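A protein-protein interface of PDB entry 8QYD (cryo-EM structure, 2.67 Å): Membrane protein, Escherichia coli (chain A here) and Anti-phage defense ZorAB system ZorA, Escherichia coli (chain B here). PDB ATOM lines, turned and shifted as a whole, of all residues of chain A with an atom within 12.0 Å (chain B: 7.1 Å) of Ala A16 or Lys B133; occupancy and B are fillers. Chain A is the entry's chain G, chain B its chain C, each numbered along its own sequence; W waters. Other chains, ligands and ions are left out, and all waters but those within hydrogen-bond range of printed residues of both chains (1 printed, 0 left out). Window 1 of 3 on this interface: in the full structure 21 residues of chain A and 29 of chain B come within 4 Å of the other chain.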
ATOM      1  N   LYS A  10      29.142 -12.249 -13.348  1.00  0.00           N
ATOM      2  CA  LYS A  10      28.034 -11.356 -13.645  1.00  0.00           C
ATOM      3  C   LYS A  10      28.381  -9.926 -13.242  1.00  0.00           C
ATOM      4  O   LYS A  10      29.140  -9.692 -12.298  1.00  0.00           O
ATOM      5  CB  LYS A  10      26.772 -11.814 -12.913  1.00  0.00           C
ATOM      6  CG  LYS A  10      26.293 -13.203 -13.305  1.00  0.00           C
ATOM      7  CD  LYS A  10      25.922 -13.277 -14.774  1.00  0.00           C
ATOM      8  CE  LYS A  10      24.697 -12.432 -15.078  1.00  0.00           C
ATOM      9  NZ  LYS A  10      23.481 -12.947 -14.389  1.00  0.00           N
ATOM     10  N   ARG A  11      27.819  -8.962 -13.969  1.00  0.00           N
ATOM     11  CA  ARG A  11      28.149  -7.573 -13.696  1.00  0.00           C
ATOM     12  C   ARG A  11      27.540  -7.126 -12.368  1.00  0.00           C
ATOM     13  O   ARG A  11      26.815  -7.865 -11.696  1.00  0.00           O
ATOM     14  CB  ARG A  11      27.644  -6.639 -14.797  1.00  0.00           C
ATOM     15  CG  ARG A  11      26.128  -6.571 -14.912  1.00  0.00           C
ATOM     16  CD  ARG A  11      25.688  -5.591 -15.994  1.00  0.00           C
ATOM     17  NE  ARG A  11      26.082  -5.953 -17.349  1.00  0.00           N
ATOM     18  CZ  ARG A  11      25.364  -6.724 -18.154  1.00  0.00           C
ATOM     19  NH1 ARG A  11      24.214  -7.248 -17.764  1.00  0.00           N
ATOM     20  NH2 ARG A  11      25.801  -6.959 -19.386  1.00  0.00           N
ATOM     21  N   ARG A  12      27.846  -5.885 -11.998  1.00  0.00           N
ATOM     22  CA  ARG A  12      27.203  -5.237 -10.865  1.00  0.00           C
ATOM     23  C   ARG A  12      25.800  -4.802 -11.269  1.00  0.00           C
ATOM     24  O   ARG A  12      25.593  -3.659 -11.690  1.00  0.00           O
ATOM     25  CB  ARG A  12      28.036  -4.042 -10.391  1.00  0.00           C
ATOM     26  CG  ARG A  12      27.444  -3.271  -9.223  1.00  0.00           C
ATOM     27  CD  ARG A  12      27.403  -4.118  -7.969  1.00  0.00           C
ATOM     28  NE  ARG A  12      28.739  -4.456  -7.499  1.00  0.00           N
ATOM     29  CZ  ARG A  12      28.995  -5.368  -6.572  1.00  0.00           C
ATOM     30  NH1 ARG A  12      28.023  -6.045  -5.985  1.00  0.00           N
ATOM     31  NH2 ARG A  12      30.256  -5.605  -6.224  1.00  0.00           N
ATOM     32  N   SER A  13      24.834  -5.710 -11.164  1.00  0.00           N
ATOM     33  CA  SER A  13      23.463  -5.458 -11.601  1.00  0.00           C
ATOM     34  C   SER A  13      22.656  -4.979 -10.401  1.00  0.00           C
ATOM     35  O   SER A  13      22.135  -5.787  -9.628  1.00  0.00           O
ATOM     36  CB  SER A  13      22.852  -6.708 -12.224  1.00  0.00           C
ATOM     37  OG  SER A  13      22.858  -7.788 -11.308  1.00  0.00           O
ATOM     38  N   ASP A  14      22.555  -3.662 -10.246  1.00  0.00           N
ATOM     39  CA  ASP A  14      21.752  -3.103  -9.169  1.00  0.00           C
ATOM     40  C   ASP A  14      20.278  -3.407  -9.403  1.00  0.00           C
ATOM     41  O   ASP A  14      19.775  -3.305 -10.525  1.00  0.00           O
ATOM     42  CB  ASP A  14      21.974  -1.593  -9.062  1.00  0.00           C
ATOM     43  CG  ASP A  14      21.394  -0.831 -10.236  1.00  0.00           C
ATOM     44  OD1 ASP A  14      21.602  -1.266 -11.388  1.00  0.00           O
ATOM     45  OD2 ASP A  14      20.725   0.198 -10.009  1.00  0.00           O
ATOM     46  N   GLU A  15      19.589  -3.792  -8.338  1.00  0.00           N
ATOM     47  CA  GLU A  15      18.189  -4.145  -8.469  1.00  0.00           C
ATOM     48  C   GLU A  15      17.336  -2.893  -8.629  1.00  0.00           C
ATOM     49  O   GLU A  15      17.756  -1.774  -8.322  1.00  0.00           O
ATOM     50  CB  GLU A  15      17.720  -4.963  -7.265  1.00  0.00           C
ATOM     51  CG  GLU A  15      17.919  -6.463  -7.428  1.00  0.00           C
ATOM     52  CD  GLU A  15      16.829  -7.122  -8.256  1.00  0.00           C
ATOM     53  OE1 GLU A  15      15.990  -6.397  -8.830  1.00  0.00           O
ATOM     54  OE2 GLU A  15      16.815  -8.368  -8.335  1.00  0.00           O
ATOM     55  N   ALA A  16      16.123  -3.094  -9.130  1.00  0.00           N
ATOM     56  CA  ALA A  16      15.211  -1.987  -9.345  1.00  0.00           C
ATOM     57  C   ALA A  16      14.613  -1.517  -8.025  1.00  0.00           C
ATOM     58  O   ALA A  16      14.755  -2.159  -6.980  1.00  0.00           O
ATOM     59  CB  ALA A  16      14.098  -2.392 -10.308  1.00  0.00           C
ATOM     60  N   GLU A  17      13.945  -0.369  -8.083  1.00  0.00           N
ATOM     61  CA  GLU A  17      13.162   0.099  -6.949  1.00  0.00           C
ATOM     62  C   GLU A  17      12.136  -0.954  -6.556  1.00  0.00           C
ATOM     63  O   GLU A  17      11.491  -1.565  -7.413  1.00  0.00           O
ATOM     64  CB  GLU A  17      12.452   1.408  -7.298  1.00  0.00           C
ATOM     65  CG  GLU A  17      13.290   2.661  -7.145  1.00  0.00           C
ATOM     66  CD  GLU A  17      13.263   3.210  -5.734  1.00  0.00           C
ATOM     67  OE1 GLU A  17      13.844   4.291  -5.504  1.00  0.00           O
ATOM     68  OE2 GLU A  17      12.657   2.565  -4.854  1.00  0.00           O
ATOM     69  N   LYS A  18      11.996  -1.176  -5.256  1.00  0.00           N
ATOM     70  CA  LYS A  18      10.991  -2.114  -4.783  1.00  0.00           C
ATOM     71  C   LYS A  18       9.606  -1.571  -5.118  1.00  0.00           C
ATOM     72  O   LYS A  18       9.270  -0.451  -4.712  1.00  0.00           O
ATOM     73  CB  LYS A  18      11.128  -2.342  -3.281  1.00  0.00           C
ATOM     74  CG  LYS A  18      12.548  -2.617  -2.837  1.00  0.00           C
ATOM     75  CD  LYS A  18      12.611  -2.925  -1.354  1.00  0.00           C
ATOM     76  CE  LYS A  18      11.887  -4.217  -1.025  1.00  0.00           C
ATOM     77  NZ  LYS A  18      11.999  -4.555   0.419  1.00  0.00           N
ATOM     78  N   PRO A  19       8.785  -2.319  -5.858  1.00  0.00           N
ATOM     79  CA  PRO A  19       7.508  -1.758  -6.322  1.00  0.00           C
ATOM     80  C   PRO A  19       6.559  -1.398  -5.199  1.00  0.00           C
ATOM     81  O   PRO A  19       5.684  -0.541  -5.387  1.00  0.00           O
ATOM     82  CB  PRO A  19       6.941  -2.878  -7.203  1.00  0.00           C
ATOM     83  CG  PRO A  19       7.558  -4.122  -6.665  1.00  0.00           C
ATOM     84  CD  PRO A  19       8.938  -3.736  -6.223  1.00  0.00           C
ATOM     85  N   PHE A  20       6.705  -2.025  -4.030  1.00  0.00           N
ATOM     86  CA  PHE A  20       5.764  -1.768  -2.950  1.00  0.00           C
ATOM     87  C   PHE A  20       5.824  -0.319  -2.501  1.00  0.00           C
ATOM     88  O   PHE A  20       4.793   0.279  -2.193  1.00  0.00           O
ATOM     89  CB  PHE A  20       6.026  -2.687  -1.761  1.00  0.00           C
ATOM     90  CG  PHE A  20       5.377  -2.211  -0.495  1.00  0.00           C
ATOM     91  CD1 PHE A  20       3.998  -2.166  -0.386  1.00  0.00           C
ATOM     92  CD2 PHE A  20       6.138  -1.786   0.575  1.00  0.00           C
ATOM     93  CE1 PHE A  20       3.394  -1.719   0.767  1.00  0.00           C
ATOM     94  CE2 PHE A  20       5.536  -1.339   1.733  1.00  0.00           C
ATOM     95  CZ  PHE A  20       4.163  -1.305   1.828  1.00  0.00           C
ATOM     96  N   TRP A  21       7.019   0.264  -2.453  1.00  0.00           N
ATOM     97  CA  TRP A  21       7.143   1.616  -1.921  1.00  0.00           C
ATOM     98  C   TRP A  21       6.530   2.647  -2.859  1.00  0.00           C
ATOM     99  O   TRP A  21       5.838   3.566  -2.409  1.00  0.00           O
ATOM    100  CB  TRP A  21       8.606   1.928  -1.639  1.00  0.00           C
ATOM    101  CG  TRP A  21       9.096   1.204  -0.444  1.00  0.00           C
ATOM    102  CD1 TRP A  21      10.047   0.232  -0.409  1.00  0.00           C
ATOM    103  CD2 TRP A  21       8.633   1.365   0.897  1.00  0.00           C
ATOM    104  NE1 TRP A  21      10.218  -0.213   0.877  1.00  0.00           N
ATOM    105  CE2 TRP A  21       9.360   0.467   1.698  1.00  0.00           C
ATOM    106  CE3 TRP A  21       7.680   2.189   1.501  1.00  0.00           C
ATOM    107  CZ2 TRP A  21       9.165   0.371   3.069  1.00  0.00           C
ATOM    108  CZ3 TRP A  21       7.488   2.090   2.858  1.00  0.00           C
ATOM    109  CH2 TRP A  21       8.228   1.191   3.628  1.00  0.00           C
ATOM    110  N   ILE A  22       6.759   2.510  -4.165  1.00  0.00           N
ATOM    111  CA  ILE A  22       6.157   3.445  -5.108  1.00  0.00           C
ATOM    112  C   ILE A  22       4.646   3.238  -5.178  1.00  0.00           C
ATOM    113  O   ILE A  22       3.879   4.205  -5.276  1.00  0.00           O
ATOM    114  CB  ILE A  22       6.836   3.329  -6.485  1.00  0.00           C
ATOM    115  CG1 ILE A  22       6.278   4.370  -7.453  1.00  0.00           C
ATOM    116  CG2 ILE A  22       6.699   1.932  -7.057  1.00  0.00           C
ATOM    117  CD1 ILE A  22       7.147   4.586  -8.662  1.00  0.00           C
ATOM    118  N   SER A  23       4.188   1.983  -5.103  1.00  0.00           N
ATOM    119  CA  SER A  23       2.750   1.728  -5.080  1.00  0.00           C
ATOM    120  C   SER A  23       2.105   2.287  -3.817  1.00  0.00           C
ATOM    121  O   SER A  23       0.986   2.808  -3.860  1.00  0.00           O
ATOM    122  CB  SER A  23       2.481   0.230  -5.199  1.00  0.00           C
ATOM    123  OG  SER A  23       2.986  -0.285  -6.415  1.00  0.00           O
ATOM    124  N   TYR B  38      10.491  -8.272 -24.843  1.00  0.00           N
ATOM    125  CA  TYR B  38      10.980  -9.117 -23.763  1.00  0.00           C
ATOM    126  C   TYR B  38      10.307 -10.482 -23.751  1.00  0.00           C
ATOM    127  O   TYR B  38      11.001 -11.500 -23.793  1.00  0.00           O
ATOM    128  CB  TYR B  38      10.784  -8.412 -22.416  1.00  0.00           C
ATOM    129  CG  TYR B  38      11.421  -9.126 -21.247  1.00  0.00           C
ATOM    130  CD1 TYR B  38      10.774 -10.175 -20.608  1.00  0.00           C
ATOM    131  CD2 TYR B  38      12.670  -8.754 -20.784  1.00  0.00           C
ATOM    132  CE1 TYR B  38      11.354 -10.829 -19.549  1.00  0.00           C
ATOM    133  CE2 TYR B  38      13.256  -9.399 -19.722  1.00  0.00           C
ATOM    134  CZ  TYR B  38      12.595 -10.437 -19.108  1.00  0.00           C
ATOM    135  OH  TYR B  38      13.178 -11.085 -18.047  1.00  0.00           O
ATOM    136  N   ASP B 124      20.531 -12.162 -20.752  1.00  0.00           N
ATOM    137  CA  ASP B 124      20.438 -10.827 -20.169  1.00  0.00           C
ATOM    138  C   ASP B 124      20.571  -9.734 -21.220  1.00  0.00           C
ATOM    139  O   ASP B 124      19.815  -8.759 -21.199  1.00  0.00           O
ATOM    140  CB  ASP B 124      21.497 -10.657 -19.084  1.00  0.00           C
ATOM    141  CG  ASP B 124      21.100 -11.317 -17.782  1.00  0.00           C
ATOM    142  OD1 ASP B 124      19.956 -11.804 -17.694  1.00  0.00           O
ATOM    143  OD2 ASP B 124      21.924 -11.355 -16.845  1.00  0.00           O
ATOM    144  N   ASN B 128      17.513  -7.368 -22.824  1.00  0.00           N
ATOM    145  CA  ASN B 128      17.636  -6.011 -22.293  1.00  0.00           C
ATOM    146  C   ASN B 128      17.092  -5.921 -20.872  1.00  0.00           C
ATOM    147  O   ASN B 128      16.364  -4.992 -20.522  1.00  0.00           O
ATOM    148  CB  ASN B 128      16.946  -4.991 -23.199  1.00  0.00           C
ATOM    149  CG  ASN B 128      17.598  -4.877 -24.556  1.00  0.00           C
ATOM    150  OD1 ASN B 128      18.636  -4.239 -24.706  1.00  0.00           O
ATOM    151  ND2 ASN B 128      16.982  -5.487 -25.558  1.00  0.00           N
ATOM    152  N   THR B 129      17.452  -6.902 -20.042  1.00  0.00           N
ATOM    153  CA  THR B 129      16.982  -6.915 -18.662  1.00  0.00           C
ATOM    154  C   THR B 129      17.479  -5.715 -17.869  1.00  0.00           C
ATOM    155  O   THR B 129      16.857  -5.352 -16.869  1.00  0.00           O
ATOM    156  CB  THR B 129      17.415  -8.202 -17.962  1.00  0.00           C
ATOM    157  OG1 THR B 129      18.832  -8.184 -17.756  1.00  0.00           O
ATOM    158  CG2 THR B 129      17.045  -9.413 -18.793  1.00  0.00           C
ATOM    159  N   GLU B 130      18.578  -5.087 -18.293  1.00  0.00           N
ATOM    160  CA  GLU B 130      19.069  -3.904 -17.597  1.00  0.00           C
ATOM    161  C   GLU B 130      18.103  -2.733 -17.699  1.00  0.00           C
ATOM    162  O   GLU B 130      18.203  -1.793 -16.905  1.00  0.00           O
ATOM    163  CB  GLU B 130      20.439  -3.498 -18.137  1.00  0.00           C
ATOM    164  CG  GLU B 130      21.573  -4.408 -17.698  1.00  0.00           C
ATOM    165  CD  GLU B 130      21.805  -4.377 -16.198  1.00  0.00           C
ATOM    166  OE1 GLU B 130      21.257  -5.245 -15.488  1.00  0.00           O
ATOM    167  OE2 GLU B 130      22.539  -3.484 -15.726  1.00  0.00           O
ATOM    168  N   PHE B 131      17.182  -2.763 -18.659  1.00  0.00           N
ATOM    169  CA  PHE B 131      16.120  -1.770 -18.760  1.00  0.00           C
ATOM    170  C   PHE B 131      14.784  -2.290 -18.249  1.00  0.00           C
ATOM    171  O   PHE B 131      14.067  -1.574 -17.548  1.00  0.00           O
ATOM    172  CB  PHE B 131      15.955  -1.302 -20.210  1.00  0.00           C
ATOM    173  CG  PHE B 131      14.660  -0.585 -20.462  1.00  0.00           C
ATOM    174  CD1 PHE B 131      14.482   0.719 -20.037  1.00  0.00           C
ATOM    175  CD2 PHE B 131      13.612  -1.222 -21.102  1.00  0.00           C
ATOM    176  CE1 PHE B 131      13.292   1.376 -20.255  1.00  0.00           C
ATOM    177  CE2 PHE B 131      12.419  -0.569 -21.319  1.00  0.00           C
ATOM    178  CZ  PHE B 131      12.259   0.731 -20.897  1.00  0.00           C
ATOM    179  N   PHE B 132      14.434  -3.529 -18.592  1.00  0.00           N
ATOM    180  CA  PHE B 132      13.081  -4.014 -18.364  1.00  0.00           C
ATOM    181  C   PHE B 132      12.803  -4.354 -16.907  1.00  0.00           C
ATOM    182  O   PHE B 132      11.633  -4.442 -16.527  1.00  0.00           O
ATOM    183  CB  PHE B 132      12.810  -5.227 -19.249  1.00  0.00           C
ATOM    184  CG  PHE B 132      12.356  -4.870 -20.632  1.00  0.00           C
ATOM    185  CD1 PHE B 132      11.083  -4.374 -20.847  1.00  0.00           C
ATOM    186  CD2 PHE B 132      13.200  -5.019 -21.716  1.00  0.00           C
ATOM    187  CE1 PHE B 132      10.662  -4.037 -22.114  1.00  0.00           C
ATOM    188  CE2 PHE B 132      12.780  -4.687 -22.987  1.00  0.00           C
ATOM    189  CZ  PHE B 132      11.508  -4.197 -23.184  1.00  0.00           C
ATOM    190  N   LYS B 133      13.832  -4.550 -16.084  1.00  0.00           N
ATOM    191  CA  LYS B 133      13.568  -4.762 -14.667  1.00  0.00           C
ATOM    192  C   LYS B 133      13.109  -3.493 -13.964  1.00  0.00           C
ATOM    193  O   LYS B 133      12.571  -3.581 -12.856  1.00  0.00           O
ATOM    194  CB  LYS B 133      14.800  -5.327 -13.960  1.00  0.00           C
ATOM    195  CG  LYS B 133      15.992  -4.399 -13.918  1.00  0.00           C
ATOM    196  CD  LYS B 133      17.140  -5.035 -13.156  1.00  0.00           C
ATOM    197  CE  LYS B 133      17.787  -6.150 -13.953  1.00  0.00           C
ATOM    198  NZ  LYS B 133      18.994  -6.698 -13.280  1.00  0.00           N
ATOM    199  N   HIS B 134      13.306  -2.327 -14.574  1.00  0.00           N
ATOM    200  CA  HIS B 134      12.854  -1.056 -14.027  1.00  0.00           C
ATOM    201  C   HIS B 134      11.551  -0.568 -14.644  1.00  0.00           C
ATOM    202  O   HIS B 134      11.078   0.510 -14.278  1.00  0.00           O
ATOM    203  CB  HIS B 134      13.943   0.005 -14.207  1.00  0.00           C
ATOM    204  CG  HIS B 134      15.276  -0.402 -13.664  1.00  0.00           C
ATOM    205  ND1 HIS B 134      16.256  -0.973 -14.444  1.00  0.00           N
ATOM    206  CD2 HIS B 134      15.792  -0.315 -12.416  1.00  0.00           C
ATOM    207  CE1 HIS B 134      17.317  -1.227 -13.699  1.00  0.00           C
ATOM    208  NE2 HIS B 134      17.062  -0.834 -12.465  1.00  0.00           N
ATOM    209  N   LEU B 135      10.970  -1.327 -15.571  1.00  0.00           N
ATOM    210  CA  LEU B 135       9.713  -0.917 -16.190  1.00  0.00           C
ATOM    211  C   LEU B 135       8.536  -0.831 -15.220  1.00  0.00           C
ATOM    212  O   LEU B 135       7.769   0.143 -15.321  1.00  0.00           O
ATOM    213  CB  LEU B 135       9.387  -1.859 -17.356  1.00  0.00           C
ATOM    214  CG  LEU B 135       8.199  -1.458 -18.228  1.00  0.00           C
ATOM    215  CD1 LEU B 135       8.490  -0.151 -18.935  1.00  0.00           C
ATOM    216  CD2 LEU B 135       7.886  -2.548 -19.231  1.00  0.00           C
ATOM    217  N   PRO B 136       8.304  -1.790 -14.310  1.00  0.00           N
ATOM    218  CA  PRO B 136       7.143  -1.660 -13.409  1.00  0.00           C
ATOM    219  C   PRO B 136       7.157  -0.397 -12.564  1.00  0.00           C
ATOM    220  O   PRO B 136       6.095   0.194 -12.310  1.00  0.00           O
ATOM    221  CB  PRO B 136       7.239  -2.922 -12.543  1.00  0.00           C
ATOM    222  CG  PRO B 136       7.981  -3.884 -13.376  1.00  0.00           C
ATOM    223  CD  PRO B 136       8.980  -3.087 -14.129  1.00  0.00           C
ATOM    224  N   GLY B 137       8.335   0.032 -12.114  1.00  0.00           N
ATOM    225  CA  GLY B 137       8.423   1.297 -11.409  1.00  0.00           C
ATOM    226  C   GLY B 137       8.031   2.467 -12.287  1.00  0.00           C
ATOM    227  O   GLY B 137       7.383   3.407 -11.829  1.00  0.00           O
ATOM    228  N   THR B 195       5.806  -7.490 -13.844  1.00  0.00           N
ATOM    229  CA  THR B 195       6.748  -8.096 -12.907  1.00  0.00           C
ATOM    230  C   THR B 195       6.602  -9.611 -12.885  1.00  0.00           C
ATOM    231  O   THR B 195       7.595 -10.344 -12.958  1.00  0.00           O
ATOM    232  CB  THR B 195       6.542  -7.525 -11.506  1.00  0.00           C
ATOM    233  OG1 THR B 195       6.593  -6.097 -11.556  1.00  0.00           O
ATOM    234  CG2 THR B 195       7.622  -8.025 -10.570  1.00  0.00           C
ATOM    235  N   GLU B 198       7.808 -11.069 -16.311  1.00  0.00           N
ATOM    236  CA  GLU B 198       9.246 -10.892 -16.456  1.00  0.00           C
ATOM    237  C   GLU B 198      10.025 -11.848 -15.569  1.00  0.00           C
ATOM    238  O   GLU B 198      10.974 -12.494 -16.023  1.00  0.00           O
ATOM    239  CB  GLU B 198       9.621  -9.456 -16.115  1.00  0.00           C
ATOM    240  CG  GLU B 198      11.079  -9.170 -16.307  1.00  0.00           C
ATOM    241  CD  GLU B 198      11.429  -7.742 -16.009  1.00  0.00           C
ATOM    242  OE1 GLU B 198      10.524  -6.972 -15.630  1.00  0.00           O
ATOM    243  OE2 GLU B 198      12.619  -7.397 -16.142  1.00  0.00           O
ATOM    244  N   LYS B 199       9.660 -11.928 -14.290  1.00  0.00           N
ATOM    245  CA  LYS B 199      10.416 -12.768 -13.374  1.00  0.00           C
ATOM    246  C   LYS B 199      10.221 -14.243 -13.696  1.00  0.00           C
ATOM    247  O   LYS B 199      11.172 -15.030 -13.619  1.00  0.00           O
ATOM    248  CB  LYS B 199      10.016 -12.452 -11.938  1.00  0.00           C
ATOM    249  CG  LYS B 199      10.428 -11.055 -11.518  1.00  0.00           C
ATOM    250  CD  LYS B 199      11.903 -10.833 -11.779  1.00  0.00           C
ATOM    251  CE  LYS B 199      12.178  -9.437 -12.307  1.00  0.00           C
ATOM    252  NZ  LYS B 199      11.644  -8.375 -11.422  1.00  0.00           N
ATOM    253  N   TYR B 206      16.816 -19.013 -17.081  1.00  0.00           N
ATOM    254  CA  TYR B 206      17.979 -19.494 -16.344  1.00  0.00           C
ATOM    255  C   TYR B 206      17.937 -21.008 -16.174  1.00  0.00           C
ATOM    256  O   TYR B 206      18.962 -21.683 -16.330  1.00  0.00           O
ATOM    257  CB  TYR B 206      18.067 -18.794 -14.991  1.00  0.00           C
ATOM    258  CG  TYR B 206      18.480 -17.344 -15.096  1.00  0.00           C
ATOM    259  CD1 TYR B 206      18.811 -16.785 -16.321  1.00  0.00           C
ATOM    260  CD2 TYR B 206      18.541 -16.535 -13.973  1.00  0.00           C
ATOM    261  CE1 TYR B 206      19.187 -15.466 -16.426  1.00  0.00           C
ATOM    262  CE2 TYR B 206      18.917 -15.211 -14.071  1.00  0.00           C
ATOM    263  CZ  TYR B 206      19.239 -14.684 -15.299  1.00  0.00           C
ATOM    264  OH  TYR B 206      19.613 -13.367 -15.402  1.00  0.00           O
HETATM  265  O   HOH W   1      10.809  -2.014 -10.743  1.00  0.00           O
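The side-chain carboxylate (OD2) of Asp B124 lies within salt-bridge range of the side-chain amino group (NZ) of Lys A10, 3.3 Å away.
The side-chain carboxylate (OE1) of Glu B130 is in salt-bridge range of the side-chain amino group (NZ) of Lys B133, 3.5 Å away.
The side-chain carboxylate (OD1) of Asp B124 sits at hydrogen-bond distance from the side-chain hydroxyl (OH) of Tyr B206 (2.8 Å).
The backbone carbonyl oxygen of Glu B130 lies within hydrogen-bond range of a ring nitrogen (ND1) of His B134.
The backbone carbonyl oxygen (O) of Asp B124 sits at hydrogen-bond distance from the backbone NH (N) of Thr B129, at 3.2 Å.
The backbone NH of Lys B133 sits at hydrogen-bond distance from the side-chain carboxylate of Glu B198, at 3.1 Å.
Arg A11 touches Glu B130 (CD to OE2, 3.8 Å).
Ser A13 touches Glu B130.
CB of Ser A13 touches NZ of Lys B133, 3.9999 Å away.
O of Lys B133 touches CB of Ala A16, at 3.2 Å.
CB of Ala A16 touches CD2 of His B134 (3.4 Å).
Gly B137 touches Ile A22 (O to CD1, 3.4 Å).
Of the printed residues of chain B, Lys A10 touches Asp B124.
Of the printed residues of chain B, Arg A11 touches Glu B130.
Printed residues of chain B within 4 Å of Ser A13: Glu B130 and Lys B133.
Pro A19 touches none of the printed residues of chain B.
Of the printed residues of chain B, Ile A22 touches Gly B137 (3.4 Å).
Printed residues of chain A within 4 Å of Asp B124: Lys A10 (3.3 Å).
Asn B128 touches none of the printed residues of chain A.
No residue of chain A comes within 4 Å of Thr B129.
Of chain A, only Arg A11 and Ser A13 come within 4 Å of Glu B130.
Phe B131 touches none of the printed residues of chain A.
Printed residues of chain A within 4 Å of Lys B133: Ser A13 and Ala A16.
No residue of chain A comes within 4 Å of Pro B136.
The nearest residue of chain B that does not touch Ala A16 is Leu B135 (6.2 Å).
The nearest printed residue of chain B that does not touch Lys A10 is Tyr B206 (4.02 Å).
Printed residues of chain B that touch a printed residue of chain A: Asp B124, Glu B130, Lys B133, His B134 and Gly B137.
Of the 14 printed residues of chain A, 5 touch a printed residue of chain B.
Printed residues of chain A that touch a printed residue of chain B: Lys A10, Arg A11, Ser A13, Ala A16 and Ile A22.
Among the printed residues, Asp or Glu carboxylates within 4 Å of a Lys or Arg side-chain nitrogen of the other chain: Lys A10 with Asp B124 (3.3 Å).
Water W1 lies within hydrogen-bond range of O of Lys B133 (3.2 Å), O of Glu A17 (3.4 Å) and N of Gly B137 (3.5 Å).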
